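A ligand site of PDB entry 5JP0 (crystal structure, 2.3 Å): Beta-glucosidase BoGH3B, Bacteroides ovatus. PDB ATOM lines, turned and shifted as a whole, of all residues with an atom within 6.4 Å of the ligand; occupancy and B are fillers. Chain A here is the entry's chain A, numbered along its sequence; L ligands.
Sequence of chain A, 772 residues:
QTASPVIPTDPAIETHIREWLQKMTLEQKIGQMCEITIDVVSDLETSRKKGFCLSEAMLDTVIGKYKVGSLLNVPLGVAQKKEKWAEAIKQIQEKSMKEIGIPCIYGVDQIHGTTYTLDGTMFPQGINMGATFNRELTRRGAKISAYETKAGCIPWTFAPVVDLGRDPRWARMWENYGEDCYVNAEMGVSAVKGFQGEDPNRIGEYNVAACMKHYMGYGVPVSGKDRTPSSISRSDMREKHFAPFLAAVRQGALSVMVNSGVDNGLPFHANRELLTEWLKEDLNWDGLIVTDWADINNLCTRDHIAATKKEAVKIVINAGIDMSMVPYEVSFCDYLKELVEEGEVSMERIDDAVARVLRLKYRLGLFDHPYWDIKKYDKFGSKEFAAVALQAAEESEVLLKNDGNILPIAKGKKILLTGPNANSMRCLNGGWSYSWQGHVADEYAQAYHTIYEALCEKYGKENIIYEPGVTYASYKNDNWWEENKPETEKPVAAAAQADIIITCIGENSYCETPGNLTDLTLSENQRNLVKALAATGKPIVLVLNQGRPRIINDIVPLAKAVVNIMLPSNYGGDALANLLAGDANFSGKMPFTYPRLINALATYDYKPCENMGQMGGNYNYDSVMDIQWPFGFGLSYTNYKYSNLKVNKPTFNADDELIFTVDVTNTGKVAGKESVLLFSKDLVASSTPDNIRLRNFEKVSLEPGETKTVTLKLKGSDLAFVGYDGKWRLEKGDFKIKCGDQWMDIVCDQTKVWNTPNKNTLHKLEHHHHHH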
ATOM      1  N   LEU A  72      12.982   0.222  18.903  1.00  0.00           N
ATOM      2  CA  LEU A  72      12.568  -1.091  19.431  1.00  0.00           C
ATOM      3  C   LEU A  72      13.715  -1.847  20.161  1.00  0.00           C
ATOM      4  O   LEU A  72      14.870  -1.434  20.118  1.00  0.00           O
ATOM      5  CB  LEU A  72      12.030  -1.983  18.308  1.00  0.00           C
ATOM      6  CG  LEU A  72      13.081  -2.720  17.457  1.00  0.00           C
ATOM      7  CD1 LEU A  72      12.606  -4.113  17.062  1.00  0.00           C
ATOM      8  CD2 LEU A  72      13.497  -1.917  16.235  1.00  0.00           C
ATOM      9  N   ASN A  73      13.331  -2.958  20.781  1.00  0.00           N
ATOM     10  CA  ASN A  73      14.208  -3.983  21.352  1.00  0.00           C
ATOM     11  C   ASN A  73      14.716  -3.669  22.765  1.00  0.00           C
ATOM     12  O   ASN A  73      14.531  -2.553  23.268  1.00  0.00           O
ATOM     13  CB  ASN A  73      15.386  -4.303  20.426  1.00  0.00           C
ATOM     14  CG  ASN A  73      15.629  -5.801  20.257  1.00  0.00           C
ATOM     15  OD1 ASN A  73      15.139  -6.633  21.025  1.00  0.00           O
ATOM     16  ND2 ASN A  73      16.393  -6.132  19.242  1.00  0.00           N
ATOM     17  N   ASP A 109       9.230  -6.909  22.193  1.00  0.00           N
ATOM     18  CA  ASP A 109       8.773  -8.288  22.210  1.00  0.00           C
ATOM     19  C   ASP A 109       8.472  -8.792  23.637  1.00  0.00           C
ATOM     20  O   ASP A 109       9.246  -9.581  24.195  1.00  0.00           O
ATOM     21  CB  ASP A 109       9.841  -9.177  21.556  1.00  0.00           C
ATOM     22  CG  ASP A 109       9.977  -8.904  20.063  1.00  0.00           C
ATOM     23  OD1 ASP A 109       9.051  -9.288  19.310  1.00  0.00           O
ATOM     24  OD2 ASP A 109      10.980  -8.289  19.642  1.00  0.00           O
ATOM     25  N   ILE A 111       6.460 -11.251  24.977  1.00  0.00           N
ATOM     26  CA  ILE A 111       5.806 -12.386  24.268  1.00  0.00           C
ATOM     27  C   ILE A 111       4.874 -13.279  25.119  1.00  0.00           C
ATOM     28  O   ILE A 111       3.881 -13.788  24.598  1.00  0.00           O
ATOM     29  CB  ILE A 111       6.881 -13.271  23.557  1.00  0.00           C
ATOM     30  CG1 ILE A 111       7.746 -12.436  22.596  1.00  0.00           C
ATOM     31  CG2 ILE A 111       6.265 -14.469  22.825  1.00  0.00           C
ATOM     32  CD1 ILE A 111       6.964 -11.541  21.643  1.00  0.00           C
ATOM     33  N   PHE A 158       4.986  -6.473  20.585  1.00  0.00           N
ATOM     34  CA  PHE A 158       4.998  -7.256  19.342  1.00  0.00           C
ATOM     35  C   PHE A 158       4.405  -8.645  19.643  1.00  0.00           C
ATOM     36  O   PHE A 158       5.110  -9.654  19.690  1.00  0.00           O
ATOM     37  CB  PHE A 158       6.398  -7.352  18.750  1.00  0.00           C
ATOM     38  CG  PHE A 158       7.012  -6.042  18.341  1.00  0.00           C
ATOM     39  CD1 PHE A 158       6.269  -5.042  17.711  1.00  0.00           C
ATOM     40  CD2 PHE A 158       8.394  -5.814  18.531  1.00  0.00           C
ATOM     41  CE1 PHE A 158       6.866  -3.840  17.326  1.00  0.00           C
ATOM     42  CE2 PHE A 158       8.990  -4.619  18.139  1.00  0.00           C
ATOM     43  CZ  PHE A 158       8.227  -3.626  17.544  1.00  0.00           C
ATOM     44  N   VAL A 161       1.173 -13.781  18.678  1.00  0.00           N
ATOM     45  CA  VAL A 161       1.523 -14.581  17.524  1.00  0.00           C
ATOM     46  C   VAL A 161       0.373 -15.543  17.190  1.00  0.00           C
ATOM     47  O   VAL A 161      -0.087 -16.297  18.056  1.00  0.00           O
ATOM     48  CB  VAL A 161       2.814 -15.388  17.773  1.00  0.00           C
ATOM     49  CG1 VAL A 161       3.203 -16.173  16.534  1.00  0.00           C
ATOM     50  CG2 VAL A 161       3.945 -14.452  18.184  1.00  0.00           C
ATOM     51  N   ARG A 172       9.628 -22.091  15.453  1.00  0.00           N
ATOM     52  CA  ARG A 172       8.665 -21.165  16.056  1.00  0.00           C
ATOM     53  C   ARG A 172       7.262 -21.781  16.260  1.00  0.00           C
ATOM     54  O   ARG A 172       6.281 -21.051  16.466  1.00  0.00           O
ATOM     55  CB  ARG A 172       8.594 -19.894  15.204  1.00  0.00           C
ATOM     56  CG  ARG A 172       9.966 -19.417  14.715  1.00  0.00           C
ATOM     57  CD  ARG A 172       9.984 -17.987  14.210  1.00  0.00           C
ATOM     58  NE  ARG A 172       9.604 -17.026  15.254  1.00  0.00           N
ATOM     59  CZ  ARG A 172       9.637 -15.697  15.100  1.00  0.00           C
ATOM     60  NH1 ARG A 172       9.274 -14.915  16.103  1.00  0.00           N
ATOM     61  NH2 ARG A 172      10.066 -15.149  13.964  1.00  0.00           N
ATOM     62  N   GLU A 175       5.365 -20.633  19.534  1.00  0.00           N
ATOM     63  CA  GLU A 175       4.990 -19.227  19.777  1.00  0.00           C
ATOM     64  C   GLU A 175       3.475 -18.977  19.579  1.00  0.00           C
ATOM     65  O   GLU A 175       2.923 -18.098  20.216  1.00  0.00           O
ATOM     66  CB  GLU A 175       5.796 -18.280  18.879  1.00  0.00           C
ATOM     67  CG  GLU A 175       7.290 -18.325  19.164  1.00  0.00           C
ATOM     68  CD  GLU A 175       8.100 -17.329  18.357  1.00  0.00           C
ATOM     69  OE1 GLU A 175       7.649 -16.197  18.133  1.00  0.00           O
ATOM     70  OE2 GLU A 175       9.225 -17.676  17.957  1.00  0.00           O
ATOM     71  N   LYS A 213       1.227 -11.120  14.592  1.00  0.00           N
ATOM     72  CA  LYS A 213       2.388 -11.682  13.890  1.00  0.00           C
ATOM     73  C   LYS A 213       2.133 -13.138  13.450  1.00  0.00           C
ATOM     74  O   LYS A 213       1.426 -13.854  14.153  1.00  0.00           O
ATOM     75  CB  LYS A 213       3.604 -11.692  14.824  1.00  0.00           C
ATOM     76  CG  LYS A 213       3.848 -10.416  15.581  1.00  0.00           C
ATOM     77  CD  LYS A 213       5.291 -10.300  16.069  1.00  0.00           C
ATOM     78  CE  LYS A 213       5.607 -11.384  17.073  1.00  0.00           C
ATOM     79  NZ  LYS A 213       6.860 -11.091  17.795  1.00  0.00           N
ATOM     80  N   HIS A 214       2.664 -13.605  12.316  1.00  0.00           N
ATOM     81  CA  HIS A 214       3.430 -12.856  11.315  1.00  0.00           C
ATOM     82  C   HIS A 214       2.647 -13.030  10.000  1.00  0.00           C
ATOM     83  O   HIS A 214       2.670 -14.109   9.409  1.00  0.00           O
ATOM     84  CB  HIS A 214       4.849 -13.415  11.157  1.00  0.00           C
ATOM     85  CG  HIS A 214       5.632 -13.461  12.426  1.00  0.00           C
ATOM     86  ND1 HIS A 214       5.410 -14.411  13.404  1.00  0.00           N
ATOM     87  CD2 HIS A 214       6.647 -12.681  12.883  1.00  0.00           C
ATOM     88  CE1 HIS A 214       6.234 -14.187  14.422  1.00  0.00           C
ATOM     89  NE2 HIS A 214       6.992 -13.144  14.121  1.00  0.00           N
ATOM     90  N   TYR A 218       3.460 -18.046   7.742  1.00  0.00           N
ATOM     91  CA  TYR A 218       4.869 -18.172   8.185  1.00  0.00           C
ATOM     92  C   TYR A 218       5.225 -19.564   8.728  1.00  0.00           C
ATOM     93  O   TYR A 218       6.379 -19.984   8.653  1.00  0.00           O
ATOM     94  CB  TYR A 218       5.122 -17.078   9.243  1.00  0.00           C
ATOM     95  CG  TYR A 218       6.514 -16.923   9.788  1.00  0.00           C
ATOM     96  CD1 TYR A 218       7.656 -17.148   9.001  1.00  0.00           C
ATOM     97  CD2 TYR A 218       6.695 -16.461  11.095  1.00  0.00           C
ATOM     98  CE1 TYR A 218       8.930 -16.962   9.519  1.00  0.00           C
ATOM     99  CE2 TYR A 218       7.970 -16.268  11.620  1.00  0.00           C
ATOM    100  CZ  TYR A 218       9.099 -16.514  10.839  1.00  0.00           C
ATOM    101  OH  TYR A 218      10.367 -16.364  11.375  1.00  0.00           O
ATOM    102  N   ARG A 227      12.017 -19.167   7.689  1.00  0.00           N
ATOM    103  CA  ARG A 227      12.230 -18.177   6.617  1.00  0.00           C
ATOM    104  C   ARG A 227      12.690 -18.807   5.291  1.00  0.00           C
ATOM    105  O   ARG A 227      13.523 -18.242   4.566  1.00  0.00           O
ATOM    106  CB  ARG A 227      13.193 -17.051   7.091  1.00  0.00           C
ATOM    107  CG  ARG A 227      12.624 -16.209   8.215  1.00  0.00           C
ATOM    108  CD  ARG A 227      13.711 -15.277   8.742  1.00  0.00           C
ATOM    109  NE  ARG A 227      13.214 -14.087   9.430  1.00  0.00           N
ATOM    110  CZ  ARG A 227      12.974 -13.957  10.750  1.00  0.00           C
ATOM    111  NH1 ARG A 227      13.130 -14.970  11.611  1.00  0.00           N
ATOM    112  NH2 ARG A 227      12.552 -12.789  11.219  1.00  0.00           N
ATOM    113  N   MET A 257       2.436  -7.188  12.020  1.00  0.00           N
ATOM    114  CA  MET A 257       3.792  -7.400  11.517  1.00  0.00           C
ATOM    115  C   MET A 257       3.778  -8.452  10.417  1.00  0.00           C
ATOM    116  O   MET A 257       3.093  -9.476  10.547  1.00  0.00           O
ATOM    117  CB  MET A 257       4.733  -7.834  12.639  1.00  0.00           C
ATOM    118  CG  MET A 257       6.192  -7.779  12.252  1.00  0.00           C
ATOM    119  SD  MET A 257       7.290  -8.373  13.549  1.00  0.00           S
ATOM    120  CE  MET A 257       7.114  -7.045  14.750  1.00  0.00           C
ATOM    121  N   SER A 260       8.363 -12.597   7.278  1.00  0.00           N
ATOM    122  CA  SER A 260       9.671 -12.441   6.645  1.00  0.00           C
ATOM    123  C   SER A 260       9.867 -13.278   5.395  1.00  0.00           C
ATOM    124  O   SER A 260      10.684 -12.942   4.547  1.00  0.00           O
ATOM    125  CB  SER A 260      10.791 -12.803   7.660  1.00  0.00           C
ATOM    126  OG  SER A 260      12.072 -12.648   7.085  1.00  0.00           O
ATOM    127  N   THR A 291       7.202  -3.842   9.247  1.00  0.00           N
ATOM    128  CA  THR A 291       7.987  -4.955   8.739  1.00  0.00           C
ATOM    129  C   THR A 291       8.498  -5.739   9.943  1.00  0.00           C
ATOM    130  O   THR A 291       8.535  -5.220  11.064  1.00  0.00           O
ATOM    131  CB  THR A 291       9.209  -4.559   7.865  1.00  0.00           C
ATOM    132  OG1 THR A 291      10.293  -4.100   8.669  1.00  0.00           O
ATOM    133  CG2 THR A 291       8.868  -3.498   6.846  1.00  0.00           C
ATOM    134  N   ASP A 292       8.892  -6.974   9.689  1.00  0.00           N
ATOM    135  CA  ASP A 292       9.765  -7.726  10.574  1.00  0.00           C
ATOM    136  C   ASP A 292      11.218  -7.271  10.308  1.00  0.00           C
ATOM    137  O   ASP A 292      11.491  -6.381   9.485  1.00  0.00           O
ATOM    138  CB  ASP A 292       9.516  -9.235  10.370  1.00  0.00           C
ATOM    139  CG  ASP A 292       9.896 -10.069  11.574  1.00  0.00           C
ATOM    140  OD1 ASP A 292      10.675  -9.558  12.398  1.00  0.00           O
ATOM    141  OD2 ASP A 292       9.443 -11.229  11.715  1.00  0.00           O
ATOM    142  N   TRP A 293      12.143  -7.894  11.026  1.00  0.00           N
ATOM    143  CA  TRP A 293      13.508  -7.402  11.202  1.00  0.00           C
ATOM    144  C   TRP A 293      14.331  -7.464   9.906  1.00  0.00           C
ATOM    145  O   TRP A 293      14.561  -8.541   9.363  1.00  0.00           O
ATOM    146  CB  TRP A 293      14.135  -8.248  12.316  1.00  0.00           C
ATOM    147  CG  TRP A 293      15.536  -7.985  12.708  1.00  0.00           C
ATOM    148  CD1 TRP A 293      16.663  -8.486  12.107  1.00  0.00           C
ATOM    149  CD2 TRP A 293      15.990  -7.223  13.836  1.00  0.00           C
ATOM    150  NE1 TRP A 293      17.784  -8.056  12.771  1.00  0.00           N
ATOM    151  CE2 TRP A 293      17.404  -7.277  13.831  1.00  0.00           C
ATOM    152  CE3 TRP A 293      15.346  -6.478  14.832  1.00  0.00           C
ATOM    153  CZ2 TRP A 293      18.186  -6.622  14.797  1.00  0.00           C
ATOM    154  CZ3 TRP A 293      16.118  -5.819  15.785  1.00  0.00           C
ATOM    155  CH2 TRP A 293      17.524  -5.906  15.756  1.00  0.00           C
ATOM    156  N   MET A 325      11.183  -1.699  10.028  1.00  0.00           N
ATOM    157  CA  MET A 325      12.115  -2.158  11.055  1.00  0.00           C
ATOM    158  C   MET A 325      13.456  -2.376  10.353  1.00  0.00           C
ATOM    159  O   MET A 325      13.789  -3.491   9.936  1.00  0.00           O
ATOM    160  CB  MET A 325      11.579  -3.405  11.723  1.00  0.00           C
ATOM    161  CG  MET A 325      12.353  -3.848  12.952  1.00  0.00           C
ATOM    162  SD  MET A 325      11.698  -5.389  13.659  1.00  0.00           S
ATOM    163  CE  MET A 325      10.069  -4.963  14.239  1.00  0.00           C
ATOM    164  N   TRP A 432      12.392 -16.119  23.864  1.00  0.00           N
ATOM    165  CA  TRP A 432      11.670 -14.899  24.274  1.00  0.00           C
ATOM    166  C   TRP A 432      11.492 -14.894  25.799  1.00  0.00           C
ATOM    167  O   TRP A 432      10.381 -14.684  26.319  1.00  0.00           O
ATOM    168  CB  TRP A 432      10.313 -14.785  23.557  1.00  0.00           C
ATOM    169  CG  TRP A 432      10.398 -14.683  22.055  1.00  0.00           C
ATOM    170  CD1 TRP A 432       9.923 -15.584  21.135  1.00  0.00           C
ATOM    171  CD2 TRP A 432      10.981 -13.617  21.316  1.00  0.00           C
ATOM    172  NE1 TRP A 432      10.185 -15.131  19.861  1.00  0.00           N
ATOM    173  CE2 TRP A 432      10.821 -13.931  19.938  1.00  0.00           C
ATOM    174  CE3 TRP A 432      11.615 -12.408  21.671  1.00  0.00           C
ATOM    175  CZ2 TRP A 432      11.306 -13.095  18.922  1.00  0.00           C
ATOM    176  CZ3 TRP A 432      12.099 -11.578  20.647  1.00  0.00           C
ATOM    177  CH2 TRP A 432      11.934 -11.929  19.287  1.00  0.00           C
ATOM    178  N   TRP A 436      16.794 -13.306  24.034  1.00  0.00           N
ATOM    179  CA  TRP A 436      16.082 -13.753  22.809  1.00  0.00           C
ATOM    180  C   TRP A 436      16.070 -15.286  22.720  1.00  0.00           C
ATOM    181  O   TRP A 436      15.010 -15.899  22.567  1.00  0.00           O
ATOM    182  CB  TRP A 436      16.727 -13.100  21.597  1.00  0.00           C
ATOM    183  CG  TRP A 436      16.275 -13.522  20.234  1.00  0.00           C
ATOM    184  CD1 TRP A 436      15.004 -13.658  19.779  1.00  0.00           C
ATOM    185  CD2 TRP A 436      17.139 -13.826  19.125  1.00  0.00           C
ATOM    186  NE1 TRP A 436      15.008 -14.043  18.464  1.00  0.00           N
ATOM    187  CE2 TRP A 436      16.304 -14.150  18.032  1.00  0.00           C
ATOM    188  CE3 TRP A 436      18.548 -13.841  18.946  1.00  0.00           C
ATOM    189  CZ2 TRP A 436      16.818 -14.485  16.771  1.00  0.00           C
ATOM    190  CZ3 TRP A 436      19.071 -14.194  17.697  1.00  0.00           C
ATOM    191  CH2 TRP A 436      18.198 -14.504  16.614  1.00  0.00           C
ATOM    192  N   GLU A 512      13.737 -18.740  16.781  1.00  0.00           N
ATOM    193  CA  GLU A 512      13.899 -18.456  15.352  1.00  0.00           C
ATOM    194  C   GLU A 512      14.970 -19.313  14.659  1.00  0.00           C
ATOM    195  O   GLU A 512      15.156 -20.497  15.003  1.00  0.00           O
ATOM    196  CB  GLU A 512      14.138 -16.968  15.121  1.00  0.00           C
ATOM    197  CG  GLU A 512      13.098 -16.081  15.745  1.00  0.00           C
ATOM    198  CD  GLU A 512      13.302 -14.632  15.383  1.00  0.00           C
ATOM    199  OE1 GLU A 512      13.584 -14.328  14.199  1.00  0.00           O
ATOM    200  OE2 GLU A 512      13.189 -13.777  16.289  1.00  0.00           O
HETATM  201  C1  LIG L   1      10.968 -11.712  14.812  1.00  0.00           C
HETATM  202  C2  LIG L   1       9.697 -11.002  15.300  1.00  0.00           C
HETATM  203  C3  LIG L   1      10.072  -9.862  16.243  1.00  0.00           C
HETATM  204  C4  LIG L   1      11.002  -8.862  15.552  1.00  0.00           C
HETATM  205  C5  LIG L   1      11.486  -7.809  16.531  1.00  0.00           C
HETATM  206  C6  LIG L   1      12.144 -10.796  14.386  1.00  0.00           C
HETATM  207  O1  LIG L   1      13.373 -11.454  14.696  1.00  0.00           O
HETATM  208  O2  LIG L   1      10.634 -12.556  13.714  1.00  0.00           O
HETATM  209  O3  LIG L   1       8.848 -11.943  15.979  1.00  0.00           O
HETATM  210  O4  LIG L   1       8.894  -9.194  16.708  1.00  0.00           O
HETATM  211  O5  LIG L   1      12.172  -9.482  14.986  1.00  0.00           O
HETATM  212  O6  LIG L   1      12.298  -8.426  17.540  1.00  0.00           O
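Leu 72 touches the ligand (CD1 to C5, 3.9 Å).
Phe 158 touches the ligand (CB to O4, 3.7 Å).
CB of Trp 293 touches O5 of the ligand (3.5 Å).
SD of Met 325 touches C5 of the ligand (3.8 Å).
Trp 432 touches the ligand.
Hydrophobic or aromatic side chains within 4 Å of the ligand: Leu 72, Phe 158, His 214, Met 257, Trp 293, Met 325 and Trp 432.
Of the 21 residues printed, 13 come within 4 Å of the ligand.
OD1 of Asp 109 lies within salt-bridge range of NZ of Lys 213, 3.2 Å away.
The guanidinium group of Arg 172 is in salt-bridge range of the side-chain carboxylate of Glu 512 (3.6 Å).
The side-chain hydroxyl (OH) of Tyr 218 sits at hydrogen-bond distance from the guanidinium group (NH2) of Arg 172, at 2.9 Å.
NE of Arg 172 lies within salt-bridge range of OE2 of Glu 175 (2.8 Å).
The side-chain carboxylate (OD2) of Asp 292 is in salt-bridge range of the guanidinium group (NH2) of Arg 227, at 3.5 Å.
The guanidinium group (NH1) of Arg 227 is in salt-bridge range of the side-chain carboxylate (OE1) of Glu 512 (2.7 Å).
The indole nitrogen (NE1) of Trp 436 lies within hydrogen-bond range of the side-chain carboxylate (OE2) of Glu 512 (2.8 Å).
The side-chain amino group of Lys 213 sits at hydrogen-bond distance from the backbone carbonyl oxygen of Phe 158 (3.0 Å).
OD2 of Asp 109 sits at hydrogen-bond distance from O6 of the ligand (2.5 Å).
The guanidinium group (NH2) of Arg 172 sits at hydrogen-bond distance from an oxygen (O2) of the ligand, at 2.7 Å.
The side-chain carboxylate of Asp 292 is in hydrogen-bond range of an oxygen (O2) of the ligand (2.7 Å).
The side-chain carboxylate of Glu 512 is in hydrogen-bond range of an oxygen (O1) of the ligand (2.8 Å).
An oxygen (O3) of the ligand lies within hydrogen-bond range of the side-chain amino group (NZ) of Lys 213 (2.8 Å).
A ring nitrogen (NE2) of His 214 lies within hydrogen-bond range of an oxygen (O3) of the ligand (2.9 Å).
O2 of the ligand sits at hydrogen-bond distance from NH2 of Arg 227 (3.2 Å).
The side-chain sulfur (SD) of Met 257 sits close to an oxygen (O4) of the ligand, at 3.6 Å.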
